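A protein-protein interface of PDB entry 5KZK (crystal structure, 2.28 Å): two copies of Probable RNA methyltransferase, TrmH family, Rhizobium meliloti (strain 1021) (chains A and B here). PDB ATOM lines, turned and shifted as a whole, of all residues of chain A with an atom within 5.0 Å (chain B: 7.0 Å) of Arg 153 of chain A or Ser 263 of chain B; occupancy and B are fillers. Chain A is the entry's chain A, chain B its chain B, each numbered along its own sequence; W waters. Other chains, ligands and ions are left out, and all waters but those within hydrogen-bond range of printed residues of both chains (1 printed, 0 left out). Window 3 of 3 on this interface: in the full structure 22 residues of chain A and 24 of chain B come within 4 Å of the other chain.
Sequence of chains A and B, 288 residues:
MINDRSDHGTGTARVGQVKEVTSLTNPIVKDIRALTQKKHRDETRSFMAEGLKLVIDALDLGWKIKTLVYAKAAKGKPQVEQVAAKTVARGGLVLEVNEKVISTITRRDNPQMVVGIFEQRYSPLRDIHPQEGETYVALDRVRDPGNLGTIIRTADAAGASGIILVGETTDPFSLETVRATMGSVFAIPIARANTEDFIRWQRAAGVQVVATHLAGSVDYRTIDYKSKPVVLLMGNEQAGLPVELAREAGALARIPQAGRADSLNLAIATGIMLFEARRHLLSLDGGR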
ATOM      1  N   GLY A 149      20.065 -14.755  -3.844  1.00  0.00           N
ATOM      2  CA  GLY A 149      20.724 -13.581  -3.320  1.00  0.00           C
ATOM      3  C   GLY A 149      22.100 -13.372  -3.905  1.00  0.00           C
ATOM      4  O   GLY A 149      22.491 -12.224  -4.220  1.00  0.00           O
ATOM      5  N   THR A 150      22.861 -14.462  -4.026  1.00  0.00           N
ATOM      6  CA  THR A 150      24.154 -14.405  -4.664  1.00  0.00           C
ATOM      7  C   THR A 150      24.084 -13.967  -6.186  1.00  0.00           C
ATOM      8  O   THR A 150      24.869 -13.154  -6.642  1.00  0.00           O
ATOM      9  CB  THR A 150      24.813 -15.733  -4.557  1.00  0.00           C
ATOM     10  OG1 THR A 150      25.058 -15.981  -3.196  1.00  0.00           O
ATOM     11  CG2 THR A 150      26.100 -15.738  -5.251  1.00  0.00           C
ATOM     12  N   ILE A 151      23.099 -14.458  -6.912  1.00  0.00           N
ATOM     13  CA  ILE A 151      22.868 -14.042  -8.301  1.00  0.00           C
ATOM     14  C   ILE A 151      22.566 -12.532  -8.337  1.00  0.00           C
ATOM     15  O   ILE A 151      23.090 -11.821  -9.138  1.00  0.00           O
ATOM     16  CB  ILE A 151      21.727 -14.922  -8.884  1.00  0.00           C
ATOM     17  CG1 ILE A 151      22.161 -16.338  -9.104  1.00  0.00           C
ATOM     18  CG2 ILE A 151      21.179 -14.424 -10.177  1.00  0.00           C
ATOM     19  CD1 ILE A 151      20.970 -17.230  -9.461  1.00  0.00           C
ATOM     20  N   ILE A 152      21.756 -12.040  -7.422  1.00  0.00           N
ATOM     21  CA  ILE A 152      21.429 -10.621  -7.433  1.00  0.00           C
ATOM     22  C   ILE A 152      22.659  -9.743  -7.235  1.00  0.00           C
ATOM     23  O   ILE A 152      22.883  -8.772  -7.908  1.00  0.00           O
ATOM     24  CB  ILE A 152      20.353 -10.298  -6.352  1.00  0.00           C
ATOM     25  CG1 ILE A 152      19.023 -10.834  -6.815  1.00  0.00           C
ATOM     26  CG2 ILE A 152      20.173  -8.760  -6.143  1.00  0.00           C
ATOM     27  CD1 ILE A 152      17.955 -10.833  -5.698  1.00  0.00           C
ATOM     28  N   ARG A 153      23.434 -10.094  -6.247  1.00  0.00           N
ATOM     29  CA  ARG A 153      24.730  -9.434  -6.059  1.00  0.00           C
ATOM     30  C   ARG A 153      25.639  -9.494  -7.255  1.00  0.00           C
ATOM     31  O   ARG A 153      26.258  -8.515  -7.671  1.00  0.00           O
ATOM     32  CB  ARG A 153      25.403 -10.130  -4.865  1.00  0.00           C
ATOM     33  CG  ARG A 153      26.677  -9.579  -4.338  1.00  0.00           C
ATOM     34  CD  ARG A 153      27.031 -10.608  -3.183  1.00  0.00           C
ATOM     35  NE  ARG A 153      28.335 -10.273  -2.635  1.00  0.00           N
ATOM     36  CZ  ARG A 153      29.039 -11.018  -1.798  1.00  0.00           C
ATOM     37  NH1 ARG A 153      28.599 -12.207  -1.356  1.00  0.00           N
ATOM     38  NH2 ARG A 153      30.217 -10.544  -1.411  1.00  0.00           N
ATOM     39  N   THR A 154      25.770 -10.668  -7.800  1.00  0.00           N
ATOM     40  CA  THR A 154      26.666 -10.869  -8.926  1.00  0.00           C
ATOM     41  C   THR A 154      26.236 -10.086 -10.198  1.00  0.00           C
ATOM     42  O   THR A 154      27.060  -9.678 -10.963  1.00  0.00           O
ATOM     43  CB  THR A 154      26.767 -12.359  -9.238  1.00  0.00           C
ATOM     44  OG1 THR A 154      27.332 -13.069  -8.103  1.00  0.00           O
ATOM     45  CG2 THR A 154      27.616 -12.609 -10.370  1.00  0.00           C
ATOM     46  N   ALA A 155      24.955 -10.079 -10.445  1.00  0.00           N
ATOM     47  CA  ALA A 155      24.347  -9.351 -11.532  1.00  0.00           C
ATOM     48  C   ALA A 155      24.605  -7.872 -11.412  1.00  0.00           C
ATOM     49  O   ALA A 155      24.894  -7.233 -12.380  1.00  0.00           O
ATOM     50  CB  ALA A 155      22.855  -9.644 -11.591  1.00  0.00           C
ATOM     51  N   ASP A 156      24.626  -7.374 -10.187  1.00  0.00           N
ATOM     52  CA  ASP A 156      24.921  -5.966  -9.851  1.00  0.00           C
ATOM     53  C   ASP A 156      26.367  -5.700 -10.058  1.00  0.00           C
ATOM     54  O   ASP A 156      26.705  -4.867 -10.917  1.00  0.00           O
ATOM     55  CB  ASP A 156      24.537  -5.736  -8.420  1.00  0.00           C
ATOM     56  CG  ASP A 156      24.664  -4.302  -7.989  1.00  0.00           C
ATOM     57  OD1 ASP A 156      24.565  -3.331  -8.762  1.00  0.00           O
ATOM     58  OD2 ASP A 156      24.836  -4.159  -6.760  1.00  0.00           O
ATOM     59  N   ALA A 157      27.253  -6.481  -9.440  1.00  0.00           N
ATOM     60  CA  ALA A 157      28.686  -6.442  -9.868  1.00  0.00           C
ATOM     61  C   ALA A 157      28.955  -6.494 -11.352  1.00  0.00           C
ATOM     62  O   ALA A 157      29.856  -5.855 -11.773  1.00  0.00           O
ATOM     63  CB  ALA A 157      29.506  -7.520  -9.241  1.00  0.00           C
ATOM     64  N   ALA A 180      22.157 -12.324   1.708  1.00  0.00           N
ATOM     65  CA  ALA A 180      23.059 -12.805   0.666  1.00  0.00           C
ATOM     66  C   ALA A 180      23.261 -11.829  -0.535  1.00  0.00           C
ATOM     67  O   ALA A 180      24.230 -11.977  -1.231  1.00  0.00           O
ATOM     68  CB  ALA A 180      22.652 -14.169   0.168  1.00  0.00           C
ATOM     69  N   THR A 181      22.386 -10.834  -0.727  1.00  0.00           N
ATOM     70  CA  THR A 181      22.651  -9.726  -1.615  1.00  0.00           C
ATOM     71  C   THR A 181      23.656  -8.741  -1.159  1.00  0.00           C
ATOM     72  O   THR A 181      24.173  -8.040  -1.989  1.00  0.00           O
ATOM     73  CB  THR A 181      21.377  -8.954  -2.081  1.00  0.00           C
ATOM     74  OG1 THR A 181      20.862  -8.094  -1.061  1.00  0.00           O
ATOM     75  CG2 THR A 181      20.296  -9.940  -2.506  1.00  0.00           C
ATOM     76  N   MET A 182      24.005  -8.713   0.132  1.00  0.00           N
ATOM     77  CA  MET A 182      24.944  -7.670   0.682  1.00  0.00           C
ATOM     78  C   MET A 182      24.578  -6.307   0.157  1.00  0.00           C
ATOM     79  O   MET A 182      25.437  -5.543  -0.288  1.00  0.00           O
ATOM     80  CB  MET A 182      26.352  -7.975   0.226  1.00  0.00           C
ATOM     81  CG  MET A 182      26.693  -9.460   0.398  1.00  0.00           C
ATOM     82  SD  MET A 182      27.061  -9.743   2.307  1.00  0.00           S
ATOM     83  CE  MET A 182      28.974 -10.282   2.092  1.00  0.00           C
ATOM     84  N   SER A 184      22.726  -5.488  -2.573  1.00  0.00           N
ATOM     85  CA  SER A 184      22.436  -5.355  -4.002  1.00  0.00           C
ATOM     86  C   SER A 184      20.945  -5.431  -4.304  1.00  0.00           C
ATOM     87  O   SER A 184      20.507  -4.995  -5.341  1.00  0.00           O
ATOM     88  CB  SER A 184      23.236  -6.338  -4.798  1.00  0.00           C
ATOM     89  OG  SER A 184      24.592  -5.933  -4.770  1.00  0.00           O
ATOM     90  N   ASN B 147      30.855 -21.616   0.852  1.00  0.00           N
ATOM     91  CA  ASN B 147      31.956 -21.254  -0.064  1.00  0.00           C
ATOM     92  C   ASN B 147      32.969 -22.368  -0.340  1.00  0.00           C
ATOM     93  O   ASN B 147      33.244 -22.659  -1.499  1.00  0.00           O
ATOM     94  CB  ASN B 147      32.720 -20.038   0.467  1.00  0.00           C
ATOM     95  CG  ASN B 147      31.972 -18.727   0.231  1.00  0.00           C
ATOM     96  OD1 ASN B 147      31.062 -18.630  -0.612  1.00  0.00           O
ATOM     97  ND2 ASN B 147      32.364 -17.692   1.012  1.00  0.00           N
ATOM     98  N   GLU B 237      38.060 -14.085   2.631  1.00  0.00           N
ATOM     99  CA  GLU B 237      36.848 -13.314   2.223  1.00  0.00           C
ATOM    100  C   GLU B 237      36.854 -11.776   2.639  1.00  0.00           C
ATOM    101  O   GLU B 237      36.285 -10.917   1.929  1.00  0.00           O
ATOM    102  CB  GLU B 237      35.546 -14.054   2.724  1.00  0.00           C
ATOM    103  CG  GLU B 237      35.208 -15.461   2.107  1.00  0.00           C
ATOM    104  CD  GLU B 237      35.501 -16.725   3.019  1.00  0.00           C
ATOM    105  OE1 GLU B 237      36.564 -16.741   3.731  1.00  0.00           O
ATOM    106  OE2 GLU B 237      34.649 -17.687   3.004  1.00  0.00           O
ATOM    107  N   ILE B 255      39.152  -9.091 -11.346  1.00  0.00           N
ATOM    108  CA  ILE B 255      37.985  -9.175 -12.210  1.00  0.00           C
ATOM    109  C   ILE B 255      37.275  -7.837 -12.340  1.00  0.00           C
ATOM    110  O   ILE B 255      36.701  -7.353 -11.359  1.00  0.00           O
ATOM    111  CB  ILE B 255      36.974 -10.236 -11.698  1.00  0.00           C
ATOM    112  CG1 ILE B 255      37.607 -11.640 -11.768  1.00  0.00           C
ATOM    113  CG2 ILE B 255      35.734 -10.207 -12.618  1.00  0.00           C
ATOM    114  CD1 ILE B 255      37.040 -12.540 -10.732  1.00  0.00           C
ATOM    115  N   GLN B 257      34.684  -5.115 -12.762  1.00  0.00           N
ATOM    116  CA  GLN B 257      33.309  -5.111 -12.325  1.00  0.00           C
ATOM    117  C   GLN B 257      32.690  -3.738 -12.748  1.00  0.00           C
ATOM    118  O   GLN B 257      33.425  -2.887 -13.195  1.00  0.00           O
ATOM    119  CB  GLN B 257      33.301  -5.335 -10.831  1.00  0.00           C
ATOM    120  CG  GLN B 257      33.352  -6.819 -10.506  1.00  0.00           C
ATOM    121  CD  GLN B 257      33.906  -7.051  -9.101  1.00  0.00           C
ATOM    122  OE1 GLN B 257      33.277  -6.700  -8.145  1.00  0.00           O
ATOM    123  NE2 GLN B 257      35.113  -7.596  -8.996  1.00  0.00           N
ATOM    124  N   ALA B 258      31.364  -3.575 -12.749  1.00  0.00           N
ATOM    125  CA  ALA B 258      30.741  -2.244 -12.867  1.00  0.00           C
ATOM    126  C   ALA B 258      30.721  -1.600 -11.433  1.00  0.00           C
ATOM    127  O   ALA B 258      30.127  -2.169 -10.470  1.00  0.00           O
ATOM    128  CB  ALA B 258      29.342  -2.365 -13.443  1.00  0.00           C
ATOM    129  N   GLY B 259      31.401  -0.457 -11.282  1.00  0.00           N
ATOM    130  CA  GLY B 259      31.588   0.199  -9.949  1.00  0.00           C
ATOM    131  C   GLY B 259      32.389  -0.570  -8.897  1.00  0.00           C
ATOM    132  O   GLY B 259      33.235   0.016  -8.196  1.00  0.00           O
ATOM    133  N   ASP B 262      35.071  -3.737  -5.807  1.00  0.00           N
ATOM    134  CA  ASP B 262      35.519  -5.149  -5.768  1.00  0.00           C
ATOM    135  C   ASP B 262      34.772  -6.032  -4.703  1.00  0.00           C
ATOM    136  O   ASP B 262      35.084  -6.002  -3.521  1.00  0.00           O
ATOM    137  CB  ASP B 262      37.047  -5.176  -5.548  1.00  0.00           C
ATOM    138  CG  ASP B 262      37.615  -6.598  -5.314  1.00  0.00           C
ATOM    139  OD1 ASP B 262      37.421  -7.148  -4.197  1.00  0.00           O
ATOM    140  OD2 ASP B 262      38.288  -7.136  -6.249  1.00  0.00           O
ATOM    141  N   SER B 263      33.816  -6.842  -5.121  1.00  0.00           N
ATOM    142  CA  SER B 263      32.938  -7.437  -4.124  1.00  0.00           C
ATOM    143  C   SER B 263      32.154  -8.683  -4.614  1.00  0.00           C
ATOM    144  O   SER B 263      30.950  -8.794  -4.376  1.00  0.00           O
ATOM    145  CB  SER B 263      31.926  -6.342  -3.710  1.00  0.00           C
ATOM    146  OG  SER B 263      31.212  -5.960  -4.896  1.00  0.00           O
ATOM    147  N   LEU B 264      32.805  -9.544  -5.367  1.00  0.00           N
ATOM    148  CA  LEU B 264      32.211 -10.848  -5.738  1.00  0.00           C
ATOM    149  C   LEU B 264      32.252 -11.789  -4.557  1.00  0.00           C
ATOM    150  O   LEU B 264      33.221 -11.807  -3.834  1.00  0.00           O
ATOM    151  CB  LEU B 264      33.005 -11.442  -6.899  1.00  0.00           C
ATOM    152  CG  LEU B 264      32.754 -10.682  -8.202  1.00  0.00           C
ATOM    153  CD1 LEU B 264      33.625 -11.326  -9.219  1.00  0.00           C
ATOM    154  CD2 LEU B 264      31.324 -10.664  -8.677  1.00  0.00           C
ATOM    155  N   ASN B 265      31.219 -12.578  -4.349  1.00  0.00           N
ATOM    156  CA  ASN B 265      31.357 -13.763  -3.410  1.00  0.00           C
ATOM    157  C   ASN B 265      32.612 -14.562  -3.818  1.00  0.00           C
ATOM    158  O   ASN B 265      32.966 -14.574  -4.998  1.00  0.00           O
ATOM    159  CB  ASN B 265      30.074 -14.540  -3.376  1.00  0.00           C
ATOM    160  CG  ASN B 265      30.270 -15.976  -2.970  1.00  0.00           C
ATOM    161  OD1 ASN B 265      30.575 -16.837  -3.805  1.00  0.00           O
ATOM    162  ND2 ASN B 265      30.145 -16.239  -1.684  1.00  0.00           N
ATOM    163  N   LEU B 266      33.395 -14.999  -2.822  1.00  0.00           N
ATOM    164  CA  LEU B 266      34.589 -15.844  -3.018  1.00  0.00           C
ATOM    165  C   LEU B 266      34.394 -17.026  -3.993  1.00  0.00           C
ATOM    166  O   LEU B 266      35.201 -17.267  -4.859  1.00  0.00           O
ATOM    167  CB  LEU B 266      35.071 -16.454  -1.690  1.00  0.00           C
ATOM    168  CG  LEU B 266      36.372 -17.344  -1.763  1.00  0.00           C
ATOM    169  CD1 LEU B 266      37.529 -16.439  -2.204  1.00  0.00           C
ATOM    170  CD2 LEU B 266      36.797 -18.032  -0.429  1.00  0.00           C
HETATM  171  O   HOH W   1      28.989 -12.218  -6.088  1.00  0.00           O
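NE of Arg 153 of chain A lies within hydrogen-bond range of O of Ser 263 of chain B (3.5 Å). The backbone carbonyl oxygen (O) of Ala 157 of chain A sits at hydrogen-bond distance from the backbone NH (N) of Ala 258 of chain B (2.9 Å).
The side-chain amide nitrogen (ND2) of Asn 265 of chain B is in hydrogen-bond range of the side-chain amide oxygen (OD1) of Asn 147 of chain B (2.8 Å). O of Ile 255 of chain B sits at hydrogen-bond distance from NE2 of Gln 257 of chain B (2.9 Å). N of Ser 263 of chain B is in hydrogen-bond range of OE1 of Gln 257 of chain B (3.1 Å).
Arg 153 of chain A touches Leu 264 of chain B (NH2 to C, 3.9 Å). NH1 of Arg 153 of chain A touches CB of Asn 265 of chain B, 3.4 Å away. Ala 157 of chain A touches Gln 257 of chain B (O to CA, 3.6 Å). Ala 157 of chain A touches Leu 264 of chain B.
Of chain B, only Ser 263, Leu 264 and Asn 265 come within 4 Å of Arg 153 of chain A. Asp 156 of chain A touches none of the printed residues of chain B. Printed residues of chain A within 4 Å of Gln 257 of chain B: Ala 157. Of the printed residues of chain A, Ala 258 of chain B touches Ala 157. Of chain A, only Arg 153 (3.5 Å) comes within 4 Å of Ser 263 of chain B. Of the printed residues of chain A, Leu 264 of chain B touches Arg 153 (3.9 Å) and Ala 157 (3.7 Å). The nearest residue of chain B that does not touch Arg 153 of chain A is Leu 266 of chain B (5.7 Å).
Of the 13 printed residues of chain A, 2 touch a printed residue of chain B. Printed residues of chain A that touch a printed residue of chain B: Arg 153 and Ala 157. Of the 11 printed residues of chain B, 5 touch a printed residue of chain A. Hydrophobic or aromatic side chains of chain B within 4 Å of the printed part of chain A: Ala 258 and Leu 264. Among the printed residues, 6 pairs touch across the chains.
No position is printed for both chains. Of the 6 pairs that touch across the chains among the printed residues, none has its exchanged pair printed and touching as well.
Water W1 lies within hydrogen-bond range of OG1 of Thr 154 of chain A and N of Asn 265 of chain B.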
